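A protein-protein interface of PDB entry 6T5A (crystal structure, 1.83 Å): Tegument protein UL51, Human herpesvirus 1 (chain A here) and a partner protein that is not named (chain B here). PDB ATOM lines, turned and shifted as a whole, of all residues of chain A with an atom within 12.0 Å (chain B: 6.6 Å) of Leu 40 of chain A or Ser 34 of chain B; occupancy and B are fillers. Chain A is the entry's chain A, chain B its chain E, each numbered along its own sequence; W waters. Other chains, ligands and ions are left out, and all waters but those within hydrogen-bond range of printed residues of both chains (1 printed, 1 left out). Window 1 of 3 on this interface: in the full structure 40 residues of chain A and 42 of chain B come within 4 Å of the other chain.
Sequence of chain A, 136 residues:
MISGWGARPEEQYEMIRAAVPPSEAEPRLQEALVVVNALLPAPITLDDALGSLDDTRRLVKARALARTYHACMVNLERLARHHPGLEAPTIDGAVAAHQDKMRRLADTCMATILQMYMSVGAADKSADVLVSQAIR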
ATOM      1  N   VAL A  36     -23.414 -13.715  -1.484  1.00  0.00           N
ATOM      2  CA  VAL A  36     -23.103 -15.107  -1.170  1.00  0.00           C
ATOM      3  C   VAL A  36     -23.607 -15.388   0.235  1.00  0.00           C
ATOM      4  O   VAL A  36     -23.352 -14.586   1.141  1.00  0.00           O
ATOM      5  CB  VAL A  36     -21.572 -15.364  -1.311  1.00  0.00           C
ATOM      6  CG1 VAL A  36     -21.203 -16.783  -0.896  1.00  0.00           C
ATOM      7  CG2 VAL A  36     -21.076 -15.082  -2.737  1.00  0.00           C
ATOM      8  N   ASN A  37     -24.342 -16.502   0.423  1.00  0.00           N
ATOM      9  CA  ASN A  37     -24.846 -16.891   1.744  1.00  0.00           C
ATOM     10  C   ASN A  37     -24.695 -18.403   1.912  1.00  0.00           C
ATOM     11  O   ASN A  37     -25.179 -19.155   1.071  1.00  0.00           O
ATOM     12  CB  ASN A  37     -26.335 -16.532   1.910  1.00  0.00           C
ATOM     13  CG  ASN A  37     -26.580 -15.063   2.044  1.00  0.00           C
ATOM     14  OD1 ASN A  37     -26.406 -14.472   3.119  1.00  0.00           O
ATOM     15  ND2 ASN A  37     -26.967 -14.443   0.945  1.00  0.00           N
ATOM     16  N   ALA A  38     -24.097 -18.849   3.022  1.00  0.00           N
ATOM     17  CA  ALA A  38     -23.985 -20.276   3.320  1.00  0.00           C
ATOM     18  C   ALA A  38     -25.384 -20.879   3.496  1.00  0.00           C
ATOM     19  O   ALA A  38     -26.297 -20.232   4.020  1.00  0.00           O
ATOM     20  CB  ALA A  38     -23.175 -20.477   4.589  1.00  0.00           C
ATOM     21  N   LEU A  39     -25.563 -22.109   3.049  1.00  0.00           N
ATOM     22  CA  LEU A  39     -26.845 -22.775   3.207  1.00  0.00           C
ATOM     23  C   LEU A  39     -27.006 -23.283   4.629  1.00  0.00           C
ATOM     24  O   LEU A  39     -28.108 -23.289   5.176  1.00  0.00           O
ATOM     25  CB  LEU A  39     -26.946 -23.949   2.209  1.00  0.00           C
ATOM     26  CG  LEU A  39     -28.171 -24.879   2.309  1.00  0.00           C
ATOM     27  CD1 LEU A  39     -29.487 -24.139   1.930  1.00  0.00           C
ATOM     28  CD2 LEU A  39     -27.947 -26.141   1.467  1.00  0.00           C
ATOM     29  N   LEU A  40     -25.905 -23.751   5.214  1.00  0.00           N
ATOM     30  CA  LEU A  40     -25.931 -24.428   6.501  1.00  0.00           C
ATOM     31  C   LEU A  40     -25.132 -23.720   7.585  1.00  0.00           C
ATOM     32  O   LEU A  40     -24.128 -23.058   7.274  1.00  0.00           O
ATOM     33  CB  LEU A  40     -25.361 -25.864   6.313  1.00  0.00           C
ATOM     34  CG  LEU A  40     -26.079 -26.757   5.288  1.00  0.00           C
ATOM     35  CD1 LEU A  40     -25.207 -27.929   4.910  1.00  0.00           C
ATOM     36  CD2 LEU A  40     -27.425 -27.261   5.829  1.00  0.00           C
ATOM     37  N   PRO A  41     -25.559 -23.883   8.864  1.00  0.00           N
ATOM     38  CA  PRO A  41     -24.807 -23.275   9.975  1.00  0.00           C
ATOM     39  C   PRO A  41     -23.497 -24.020  10.239  1.00  0.00           C
ATOM     40  O   PRO A  41     -23.486 -25.260  10.327  1.00  0.00           O
ATOM     41  CB  PRO A  41     -25.752 -23.436  11.173  1.00  0.00           C
ATOM     42  CG  PRO A  41     -26.556 -24.675  10.845  1.00  0.00           C
ATOM     43  CD  PRO A  41     -26.742 -24.641   9.354  1.00  0.00           C
ATOM     44  N   ALA A  42     -22.392 -23.257  10.383  1.00  0.00           N
ATOM     45  CA  ALA A  42     -21.067 -23.823  10.668  1.00  0.00           C
ATOM     46  C   ALA A  42     -21.090 -24.518  12.046  1.00  0.00           C
ATOM     47  O   ALA A  42     -21.785 -24.034  12.945  1.00  0.00           O
ATOM     48  CB  ALA A  42     -20.009 -22.708  10.656  1.00  0.00           C
ATOM     49  N   PRO A  43     -20.380 -25.655  12.241  1.00  0.00           N
ATOM     50  CA  PRO A  43     -19.496 -26.348  11.285  1.00  0.00           C
ATOM     51  C   PRO A  43     -20.184 -27.477  10.495  1.00  0.00           C
ATOM     52  O   PRO A  43     -19.494 -28.392  10.051  1.00  0.00           O
ATOM     53  CB  PRO A  43     -18.393 -26.877  12.207  1.00  0.00           C
ATOM     54  CG  PRO A  43     -19.177 -27.296  13.455  1.00  0.00           C
ATOM     55  CD  PRO A  43     -20.356 -26.332  13.555  1.00  0.00           C
ATOM     56  N   ILE A  44     -21.534 -27.440  10.339  1.00  0.00           N
ATOM     57  CA  ILE A  44     -22.276 -28.499   9.634  1.00  0.00           C
ATOM     58  C   ILE A  44     -21.921 -28.451   8.156  1.00  0.00           C
ATOM     59  O   ILE A  44     -22.001 -27.387   7.537  1.00  0.00           O
ATOM     60  CB  ILE A  44     -23.835 -28.448   9.862  1.00  0.00           C
ATOM     61  CG1 ILE A  44     -24.220 -28.422  11.363  1.00  0.00           C
ATOM     62  CG2 ILE A  44     -24.584 -29.580   9.098  1.00  0.00           C
ATOM     63  CD1 ILE A  44     -23.752 -29.649  12.249  1.00  0.00           C
ATOM     64  N   THR A  45     -21.532 -29.609   7.603  1.00  0.00           N
ATOM     65  CA  THR A  45     -21.134 -29.708   6.193  1.00  0.00           C
ATOM     66  C   THR A  45     -22.322 -30.178   5.350  1.00  0.00           C
ATOM     67  O   THR A  45     -23.289 -30.730   5.889  1.00  0.00           O
ATOM     68  CB  THR A  45     -19.950 -30.684   6.037  1.00  0.00           C
ATOM     69  OG1 THR A  45     -20.396 -32.028   6.269  1.00  0.00           O
ATOM     70  CG2 THR A  45     -18.757 -30.340   6.933  1.00  0.00           C
ATOM     71  N   LEU A  46     -22.221 -30.024   4.021  1.00  0.00           N
ATOM     72  CA  LEU A  46     -23.253 -30.523   3.119  1.00  0.00           C
ATOM     73  C   LEU A  46     -23.406 -32.058   3.262  1.00  0.00           C
ATOM     74  O   LEU A  46     -24.544 -32.543   3.281  1.00  0.00           O
ATOM     75  CB  LEU A  46     -22.939 -30.092   1.679  1.00  0.00           C
ATOM     76  CG  LEU A  46     -23.879 -30.572   0.566  1.00  0.00           C
ATOM     77  CD1 LEU A  46     -25.360 -30.139   0.810  1.00  0.00           C
ATOM     78  CD2 LEU A  46     -23.373 -30.074  -0.763  1.00  0.00           C
ATOM     79  N   ASP A  47     -22.269 -32.808   3.410  1.00  0.00           N
ATOM     80  CA  ASP A  47     -22.285 -34.261   3.602  1.00  0.00           C
ATOM     81  C   ASP A  47     -23.066 -34.620   4.866  1.00  0.00           C
ATOM     82  O   ASP A  47     -23.800 -35.606   4.871  1.00  0.00           O
ATOM     83  CB  ASP A  47     -20.854 -34.826   3.701  1.00  0.00           C
ATOM     84  CG  ASP A  47     -20.788 -36.342   3.688  1.00  0.00           C
ATOM     85  OD1 ASP A  47     -21.162 -36.945   2.659  1.00  0.00           O
ATOM     86  OD2 ASP A  47     -20.339 -36.927   4.698  1.00  0.00           O
ATOM     87  N   ASP A  48     -22.887 -33.830   5.955  1.00  0.00           N
ATOM     88  CA  ASP A  48     -23.588 -34.073   7.227  1.00  0.00           C
ATOM     89  C   ASP A  48     -25.099 -33.940   7.046  1.00  0.00           C
ATOM     90  O   ASP A  48     -25.849 -34.776   7.524  1.00  0.00           O
ATOM     91  CB  ASP A  48     -23.174 -33.050   8.289  1.00  0.00           C
ATOM     92  CG  ASP A  48     -21.793 -33.178   8.883  1.00  0.00           C
ATOM     93  OD1 ASP A  48     -21.227 -34.297   8.841  1.00  0.00           O
ATOM     94  OD2 ASP A  48     -21.291 -32.164   9.429  1.00  0.00           O
ATOM     95  N   ALA A  49     -25.537 -32.840   6.417  1.00  0.00           N
ATOM     96  CA  ALA A  49     -26.953 -32.576   6.232  1.00  0.00           C
ATOM     97  C   ALA A  49     -27.586 -33.539   5.234  1.00  0.00           C
ATOM     98  O   ALA A  49     -28.712 -33.955   5.465  1.00  0.00           O
ATOM     99  CB  ALA A  49     -27.171 -31.116   5.844  1.00  0.00           C
ATOM    100  N   LEU A  50     -26.849 -33.965   4.173  1.00  0.00           N
ATOM    101  CA  LEU A  50     -27.374 -34.955   3.215  1.00  0.00           C
ATOM    102  C   LEU A  50     -27.476 -36.338   3.875  1.00  0.00           C
ATOM    103  O   LEU A  50     -28.428 -37.066   3.602  1.00  0.00           O
ATOM    104  CB  LEU A  50     -26.517 -35.057   1.924  1.00  0.00           C
ATOM    105  CG  LEU A  50     -26.677 -33.917   0.875  1.00  0.00           C
ATOM    106  CD1 LEU A  50     -25.605 -34.018  -0.192  1.00  0.00           C
ATOM    107  CD2 LEU A  50     -28.033 -33.962   0.198  1.00  0.00           C
ATOM    108  N   GLY A  51     -26.510 -36.671   4.743  1.00  0.00           N
ATOM    109  CA  GLY A  51     -26.508 -37.934   5.497  1.00  0.00           C
ATOM    110  C   GLY A  51     -27.679 -37.971   6.464  1.00  0.00           C
ATOM    111  O   GLY A  51     -28.339 -39.002   6.607  1.00  0.00           O
ATOM    112  N   SER A  52     -27.994 -36.806   7.078  1.00  0.00           N
ATOM    113  CA  SER A  52     -29.133 -36.666   7.992  1.00  0.00           C
ATOM    114  C   SER A  52     -30.439 -36.802   7.229  1.00  0.00           C
ATOM    115  O   SER A  52     -31.326 -37.506   7.686  1.00  0.00           O
ATOM    116  CB  SER A  52     -29.094 -35.335   8.729  1.00  0.00           C
ATOM    117  OG  SER A  52     -30.139 -35.335   9.695  1.00  0.00           O
ATOM    118  N   LEU A  53     -30.540 -36.180   6.042  1.00  0.00           N
ATOM    119  CA  LEU A  53     -31.757 -36.280   5.236  1.00  0.00           C
ATOM    120  C   LEU A  53     -32.009 -37.747   4.847  1.00  0.00           C
ATOM    121  O   LEU A  53     -33.149 -38.184   4.877  1.00  0.00           O
ATOM    122  CB  LEU A  53     -31.649 -35.373   4.002  1.00  0.00           C
ATOM    123  CG  LEU A  53     -32.865 -35.261   3.070  1.00  0.00           C
ATOM    124  CD1 LEU A  53     -34.084 -34.665   3.794  1.00  0.00           C
ATOM    125  CD2 LEU A  53     -32.522 -34.380   1.858  1.00  0.00           C
ATOM    126  N   ASP A  54     -30.944 -38.502   4.537  1.00  0.00           N
ATOM    127  CA  ASP A  54     -31.038 -39.909   4.162  1.00  0.00           C
ATOM    128  C   ASP A  54     -31.433 -40.773   5.352  1.00  0.00           C
ATOM    129  O   ASP A  54     -32.276 -41.648   5.199  1.00  0.00           O
ATOM    130  CB  ASP A  54     -29.722 -40.412   3.546  1.00  0.00           C
ATOM    131  CG  ASP A  54     -29.902 -41.781   2.914  1.00  0.00           C
ATOM    132  OD1 ASP A  54     -30.590 -41.867   1.874  1.00  0.00           O
ATOM    133  OD2 ASP A  54     -29.384 -42.764   3.478  1.00  0.00           O
ATOM    134  N   THR A  56     -33.046 -39.737   8.106  1.00  0.00           N
ATOM    135  CA  THR A  56     -34.413 -39.337   8.434  1.00  0.00           C
ATOM    136  C   THR A  56     -35.405 -40.013   7.511  1.00  0.00           C
ATOM    137  O   THR A  56     -36.408 -40.541   8.003  1.00  0.00           O
ATOM    138  CB  THR A  56     -34.564 -37.805   8.422  1.00  0.00           C
ATOM    139  OG1 THR A  56     -33.721 -37.292   9.430  1.00  0.00           O
ATOM    140  CG2 THR A  56     -35.991 -37.346   8.726  1.00  0.00           C
ATOM    141  N   ARG A  57     -35.122 -40.042   6.190  1.00  0.00           N
ATOM    142  CA  ARG A  57     -36.027 -40.716   5.244  1.00  0.00           C
ATOM    143  C   ARG A  57     -36.130 -42.231   5.527  1.00  0.00           C
ATOM    144  O   ARG A  57     -37.236 -42.780   5.490  1.00  0.00           O
ATOM    145  CB  ARG A  57     -35.670 -40.390   3.782  1.00  0.00           C
ATOM    146  CG  ARG A  57     -36.116 -38.950   3.447  1.00  0.00           C
ATOM    147  CD  ARG A  57     -35.645 -38.393   2.116  1.00  0.00           C
ATOM    148  NE  ARG A  57     -36.180 -37.044   1.894  1.00  0.00           N
ATOM    149  CZ  ARG A  57     -35.821 -36.246   0.891  1.00  0.00           C
ATOM    150  NH1 ARG A  57     -34.910 -36.646   0.008  1.00  0.00           N
ATOM    151  NH2 ARG A  57     -36.363 -35.036   0.769  1.00  0.00           N
ATOM    152  N   ALA B  29     -35.291 -28.124  -2.821  1.00  0.00           N
ATOM    153  CA  ALA B  29     -34.322 -29.193  -2.536  1.00  0.00           C
ATOM    154  C   ALA B  29     -33.321 -28.723  -1.470  1.00  0.00           C
ATOM    155  O   ALA B  29     -33.024 -29.468  -0.540  1.00  0.00           O
ATOM    156  CB  ALA B  29     -33.599 -29.614  -3.811  1.00  0.00           C
ATOM    157  N   ALA B  30     -32.848 -27.461  -1.574  1.00  0.00           N
ATOM    158  CA  ALA B  30     -31.894 -26.894  -0.610  1.00  0.00           C
ATOM    159  C   ALA B  30     -32.553 -26.713   0.759  1.00  0.00           C
ATOM    160  O   ALA B  30     -31.915 -26.966   1.783  1.00  0.00           O
ATOM    161  CB  ALA B  30     -31.370 -25.560  -1.121  1.00  0.00           C
ATOM    162  N   GLU B  31     -33.827 -26.269   0.780  1.00  0.00           N
ATOM    163  CA  GLU B  31     -34.579 -26.098   2.031  1.00  0.00           C
ATOM    164  C   GLU B  31     -34.742 -27.436   2.778  1.00  0.00           C
ATOM    165  O   GLU B  31     -34.612 -27.457   4.003  1.00  0.00           O
ATOM    166  CB  GLU B  31     -35.939 -25.454   1.765  1.00  0.00           C
ATOM    167  CG  GLU B  31     -35.815 -23.948   1.615  1.00  0.00           C
ATOM    168  CD  GLU B  31     -37.026 -23.172   1.133  1.00  0.00           C
ATOM    169  OE1 GLU B  31     -38.041 -23.796   0.746  1.00  0.00           O
ATOM    170  OE2 GLU B  31     -36.945 -21.922   1.131  1.00  0.00           O
ATOM    171  N   ALA B  32     -34.978 -28.548   2.052  1.00  0.00           N
ATOM    172  CA  ALA B  32     -35.116 -29.881   2.680  1.00  0.00           C
ATOM    173  C   ALA B  32     -33.808 -30.290   3.370  1.00  0.00           C
ATOM    174  O   ALA B  32     -33.832 -30.872   4.449  1.00  0.00           O
ATOM    175  CB  ALA B  32     -35.524 -30.938   1.653  1.00  0.00           C
ATOM    176  N   ILE B  33     -32.664 -29.933   2.769  1.00  0.00           N
ATOM    177  CA  ILE B  33     -31.343 -30.207   3.332  1.00  0.00           C
ATOM    178  C   ILE B  33     -31.117 -29.321   4.569  1.00  0.00           C
ATOM    179  O   ILE B  33     -30.769 -29.855   5.631  1.00  0.00           O
ATOM    180  CB  ILE B  33     -30.250 -30.015   2.236  1.00  0.00           C
ATOM    181  CG1 ILE B  33     -30.454 -31.021   1.073  1.00  0.00           C
ATOM    182  CG2 ILE B  33     -28.832 -30.077   2.806  1.00  0.00           C
ATOM    183  CD1 ILE B  33     -29.764 -30.592  -0.273  1.00  0.00           C
ATOM    184  N   SER B  34     -31.318 -27.982   4.452  1.00  0.00           N
ATOM    185  CA  SER B  34     -31.108 -27.086   5.602  1.00  0.00           C
ATOM    186  C   SER B  34     -32.067 -27.352   6.772  1.00  0.00           C
ATOM    187  O   SER B  34     -31.694 -27.144   7.930  1.00  0.00           O
ATOM    188  CB  SER B  34     -31.142 -25.618   5.187  1.00  0.00           C
ATOM    189  OG  SER B  34     -32.461 -25.228   4.862  1.00  0.00           O
ATOM    190  N   GLN B  35     -33.275 -27.863   6.478  1.00  0.00           N
ATOM    191  CA  GLN B  35     -34.266 -28.194   7.511  1.00  0.00           C
ATOM    192  C   GLN B  35     -33.827 -29.337   8.430  1.00  0.00           C
ATOM    193  O   GLN B  35     -34.392 -29.487   9.505  1.00  0.00           O
ATOM    194  CB  GLN B  35     -35.640 -28.458   6.900  1.00  0.00           C
ATOM    195  CG  GLN B  35     -36.456 -27.164   6.853  1.00  0.00           C
ATOM    196  CD  GLN B  35     -37.527 -27.127   5.795  1.00  0.00           C
ATOM    197  OE1 GLN B  35     -38.314 -28.064   5.624  1.00  0.00           O
ATOM    198  NE2 GLN B  35     -37.594 -26.016   5.077  1.00  0.00           N
ATOM    199  N   GLN B  36     -32.756 -30.083   8.053  1.00  0.00           N
ATOM    200  CA  GLN B  36     -32.206 -31.149   8.898  1.00  0.00           C
ATOM    201  C   GLN B  36     -31.384 -30.573  10.051  1.00  0.00           C
ATOM    202  O   GLN B  36     -31.064 -31.307  10.977  1.00  0.00           O
ATOM    203  CB  GLN B  36     -31.358 -32.127   8.064  1.00  0.00           C
ATOM    204  CG  GLN B  36     -32.226 -32.999   7.129  1.00  0.00           C
ATOM    205  CD  GLN B  36     -33.115 -33.913   7.917  1.00  0.00           C
ATOM    206  OE1 GLN B  36     -32.658 -34.734   8.705  1.00  0.00           O
ATOM    207  NE2 GLN B  36     -34.412 -33.788   7.727  1.00  0.00           N
ATOM    208  N   THR B  37     -31.040 -29.270  10.003  1.00  0.00           N
ATOM    209  CA  THR B  37     -30.234 -28.647  11.059  1.00  0.00           C
ATOM    210  C   THR B  37     -31.130 -27.976  12.090  1.00  0.00           C
ATOM    211  O   THR B  37     -32.202 -27.460  11.761  1.00  0.00           O
ATOM    212  CB  THR B  37     -29.173 -27.671  10.486  1.00  0.00           C
ATOM    213  OG1 THR B  37     -29.829 -26.561   9.863  1.00  0.00           O
ATOM    214  CG2 THR B  37     -28.208 -28.342   9.528  1.00  0.00           C
ATOM    215  N   LEU B  38     -30.680 -27.982  13.351  1.00  0.00           N
ATOM    216  CA  LEU B  38     -31.424 -27.349  14.427  1.00  0.00           C
ATOM    217  C   LEU B  38     -30.442 -27.053  15.521  1.00  0.00           C
ATOM    218  O   LEU B  38     -29.324 -27.578  15.518  1.00  0.00           O
ATOM    219  CB  LEU B  38     -32.587 -28.252  14.958  1.00  0.00           C
ATOM    220  CG  LEU B  38     -32.229 -29.548  15.740  1.00  0.00           C
ATOM    221  CD1 LEU B  38     -33.405 -30.011  16.569  1.00  0.00           C
ATOM    222  CD2 LEU B  38     -31.756 -30.689  14.805  1.00  0.00           C
ATOM    223  N   ARG B 180     -31.062 -16.144   8.122  1.00  0.00           N
ATOM    224  CA  ARG B 180     -30.625 -17.515   8.363  1.00  0.00           C
ATOM    225  C   ARG B 180     -30.641 -17.948   9.826  1.00  0.00           C
ATOM    226  O   ARG B 180     -31.061 -19.071  10.126  1.00  0.00           O
ATOM    227  CB  ARG B 180     -29.237 -17.728   7.748  1.00  0.00           C
ATOM    228  CG  ARG B 180     -29.095 -17.382   6.246  1.00  0.00           C
ATOM    229  CD  ARG B 180     -29.777 -18.366   5.323  1.00  0.00           C
ATOM    230  NE  ARG B 180     -28.925 -18.723   4.184  1.00  0.00           N
ATOM    231  CZ  ARG B 180     -29.376 -19.231   3.041  1.00  0.00           C
ATOM    232  NH1 ARG B 180     -30.677 -19.419   2.858  1.00  0.00           N
ATOM    233  NH2 ARG B 180     -28.533 -19.541   2.069  1.00  0.00           N
ATOM    234  N   LEU B 184     -33.173 -20.565  11.664  1.00  0.00           N
ATOM    235  CA  LEU B 184     -32.604 -21.690  12.397  1.00  0.00           C
ATOM    236  C   LEU B 184     -33.292 -21.840  13.756  1.00  0.00           C
ATOM    237  O   LEU B 184     -33.695 -22.951  14.108  1.00  0.00           O
ATOM    238  CB  LEU B 184     -31.071 -21.523  12.545  1.00  0.00           C
ATOM    239  CG  LEU B 184     -30.319 -22.512  13.461  1.00  0.00           C
ATOM    240  CD1 LEU B 184     -30.581 -23.998  13.060  1.00  0.00           C
ATOM    241  CD2 LEU B 184     -28.831 -22.226  13.442  1.00  0.00           C
ATOM    242  N   ARG B 187     -37.125 -23.026  13.110  1.00  0.00           N
ATOM    243  CA  ARG B 187     -37.298 -24.454  12.819  1.00  0.00           C
ATOM    244  C   ARG B 187     -36.912 -25.323  14.017  1.00  0.00           C
ATOM    245  O   ARG B 187     -37.538 -26.359  14.222  1.00  0.00           O
ATOM    246  CB  ARG B 187     -36.621 -24.891  11.516  1.00  0.00           C
ATOM    247  CG  ARG B 187     -35.121 -25.062  11.590  1.00  0.00           C
ATOM    248  CD  ARG B 187     -34.609 -25.623  10.280  1.00  0.00           C
ATOM    249  NE  ARG B 187     -33.179 -25.380  10.158  1.00  0.00           N
ATOM    250  CZ  ARG B 187     -32.652 -24.319   9.573  1.00  0.00           C
ATOM    251  NH1 ARG B 187     -33.434 -23.400   9.025  1.00  0.00           N
ATOM    252  NH2 ARG B 187     -31.338 -24.174   9.515  1.00  0.00           N
ATOM    253  N   TRP B 191     -39.228 -28.314  15.531  1.00  0.00           N
ATOM    254  CA  TRP B 191     -38.771 -29.679  15.816  1.00  0.00           C
ATOM    255  C   TRP B 191     -39.113 -30.036  17.269  1.00  0.00           C
ATOM    256  O   TRP B 191     -39.638 -31.110  17.525  1.00  0.00           O
ATOM    257  CB  TRP B 191     -37.239 -29.805  15.656  1.00  0.00           C
ATOM    258  CG  TRP B 191     -36.749 -30.011  14.249  1.00  0.00           C
ATOM    259  CD1 TRP B 191     -36.002 -29.138  13.505  1.00  0.00           C
ATOM    260  CD2 TRP B 191     -36.900 -31.200  13.451  1.00  0.00           C
ATOM    261  NE1 TRP B 191     -35.695 -29.698  12.285  1.00  0.00           N
ATOM    262  CE2 TRP B 191     -36.217 -30.976  12.231  1.00  0.00           C
ATOM    263  CE3 TRP B 191     -37.541 -32.440  13.650  1.00  0.00           C
ATOM    264  CZ2 TRP B 191     -36.192 -31.924  11.202  1.00  0.00           C
ATOM    265  CZ3 TRP B 191     -37.490 -33.395  12.643  1.00  0.00           C
ATOM    266  CH2 TRP B 191     -36.813 -33.144  11.439  1.00  0.00           C
ATOM    267  N   LEU B 291     -23.061 -17.970  12.332  1.00  0.00           N
ATOM    268  CA  LEU B 291     -23.031 -19.364  11.834  1.00  0.00           C
ATOM    269  C   LEU B 291     -23.103 -19.493  10.315  1.00  0.00           C
ATOM    270  O   LEU B 291     -22.597 -20.465   9.762  1.00  0.00           O
ATOM    271  CB  LEU B 291     -24.155 -20.221  12.458  1.00  0.00           C
ATOM    272  CG  LEU B 291     -24.084 -20.472  13.969  1.00  0.00           C
ATOM    273  CD1 LEU B 291     -25.039 -21.569  14.386  1.00  0.00           C
ATOM    274  CD2 LEU B 291     -22.660 -20.769  14.441  1.00  0.00           C
ATOM    275  N   PHE B 292     -23.755 -18.529   9.653  1.00  0.00           N
ATOM    276  CA  PHE B 292     -23.936 -18.548   8.206  1.00  0.00           C
ATOM    277  C   PHE B 292     -23.067 -17.514   7.530  1.00  0.00           C
ATOM    278  O   PHE B 292     -23.352 -16.321   7.600  1.00  0.00           O
ATOM    279  CB  PHE B 292     -25.411 -18.327   7.855  1.00  0.00           C
ATOM    280  CG  PHE B 292     -26.355 -19.366   8.402  1.00  0.00           C
ATOM    281  CD1 PHE B 292     -26.877 -19.250   9.687  1.00  0.00           C
ATOM    282  CD2 PHE B 292     -26.809 -20.408   7.600  1.00  0.00           C
ATOM    283  CE1 PHE B 292     -27.809 -20.174  10.166  1.00  0.00           C
ATOM    284  CE2 PHE B 292     -27.749 -21.324   8.078  1.00  0.00           C
ATOM    285  CZ  PHE B 292     -28.234 -21.207   9.362  1.00  0.00           C
ATOM    286  N   TYR B 293     -21.981 -17.966   6.895  1.00  0.00           N
ATOM    287  CA  TYR B 293     -21.093 -17.071   6.163  1.00  0.00           C
ATOM    288  C   TYR B 293     -21.888 -16.233   5.164  1.00  0.00           C
ATOM    289  O   TYR B 293     -22.765 -16.754   4.467  1.00  0.00           O
ATOM    290  CB  TYR B 293     -20.024 -17.875   5.391  1.00  0.00           C
ATOM    291  CG  TYR B 293     -19.147 -16.996   4.523  1.00  0.00           C
ATOM    292  CD1 TYR B 293     -18.121 -16.237   5.078  1.00  0.00           C
ATOM    293  CD2 TYR B 293     -19.388 -16.869   3.158  1.00  0.00           C
ATOM    294  CE1 TYR B 293     -17.349 -15.377   4.292  1.00  0.00           C
ATOM    295  CE2 TYR B 293     -18.622 -16.016   2.364  1.00  0.00           C
ATOM    296  CZ  TYR B 293     -17.590 -15.290   2.933  1.00  0.00           C
ATOM    297  OH  TYR B 293     -16.822 -14.475   2.138  1.00  0.00           O
HETATM  298  O   HOH W   1     -30.428 -21.775   4.565  1.00  0.00           O
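OG1 of Thr 56 of chain A is in hydrogen-bond range of OE1 of Gln 36 of chain B (2.9 Å). O of Tyr 293 of chain B is in hydrogen-bond range of N of Ala 38 of chain A, 2.9 Å away. The backbone NH (N) of Ala 42 of chain A sits at hydrogen-bond distance from the backbone carbonyl oxygen (O) of Leu 291 of chain B (2.9 Å). The guanidinium group (NE) of Arg 180 of chain B is in hydrogen-bond range of the backbone carbonyl oxygen (O) of Ala 38 of chain A (3.0 Å). The side-chain amide oxygen (OE1) of Gln 36 of chain B is in hydrogen-bond range of the side-chain hydroxyl (OG) of Ser 52 of chain A (2.8 Å).
The backbone carbonyl oxygen of Thr 37 of chain B is in hydrogen-bond range of the guanidinium group of Arg 187 of chain B, at 2.8 Å. NE of Arg 187 of chain B is in hydrogen-bond range of O of Ser 34 of chain B, 3.2 Å away. OG1 of Thr 37 of chain B sits at hydrogen-bond distance from O of Ser 34 of chain B, 2.7 Å away. O of Glu 31 of chain B lies within hydrogen-bond range of OG of Ser 34 of chain B. O of Ser 52 of chain A sits at hydrogen-bond distance from OG1 of Thr 56 of chain A.
Arg 180 of chain B touches Asn 37 of chain A. Asn 37 of chain A touches Tyr 293 of chain B. Ala 38 of chain A touches Phe 292 of chain B. O of Leu 39 of chain A touches CB of Ser 34 of chain B, 3.8 Å away. O of Leu 39 of chain A touches CE2 of Phe 292 of chain B, at 3.5 Å. Ser 34 of chain B touches Leu 40 of chain A. Leu 40 of chain A touches Leu 291 of chain B. OG1 of Thr 37 of chain B touches CD of Pro 41 of chain A, 3.7 Å away. O of Leu 291 of chain B touches CA of Pro 41 of chain A, at 3.6 Å. CG2 of Ile 33 of chain B touches CB of Ala 49 of chain A, 3.6 Å away.
Leu 40 of chain A touches four residues of chain B. Printed residues of chain B within 4 Å of Ile 44 of chain A: Thr 37. Of the printed residues of chain B, Leu 50 of chain A touches Ile 33. Printed residues of chain B within 4 Å of Ser 52 of chain A: Gln 36. Asp 54 of chain A touches none of the printed residues of chain B. Arg 57 of chain A touches none of the printed residues of chain B. No residue of chain A comes within 4 Å of Glu 31 of chain B. Ala 32 of chain B touches just one residue of chain A: Leu 53 (3.9 Å). Ser 34 of chain B touches two residues of chain A. Printed residues of chain A within 4 Å of Gln 36 of chain B: Ser 52 (2.8 Å), Leu 53 (3.7 Å) and Thr 56 (2.9 Å). Thr 37 of chain B touches three residues of chain A. Leu 291 of chain B touches just these residues of chain A: Leu 40, Pro 41 and Ala 42.
Printed residues of chain B that touch a printed residue of chain A: Ala 30, Ala 32, Ile 33, Ser 34, Gln 36, Thr 37, Arg 180, Leu 291, Phe 292 and Tyr 293. Hydrophobic or aromatic side chains of chain B that line the printed part of chain A: Ala 30, Ile 33, Leu 291 and Phe 292. Along chain A the printed residues that touch a printed residue of chain B span positions 37 to 56. Among the printed residues, 24 pairs touch across the chains.
Water W1 lies within hydrogen-bond range of the backbone carbonyl oxygen of Leu 39 of chain A (2.8 Å) and the guanidinium group of Arg 180 of chain B (2.9 Å).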
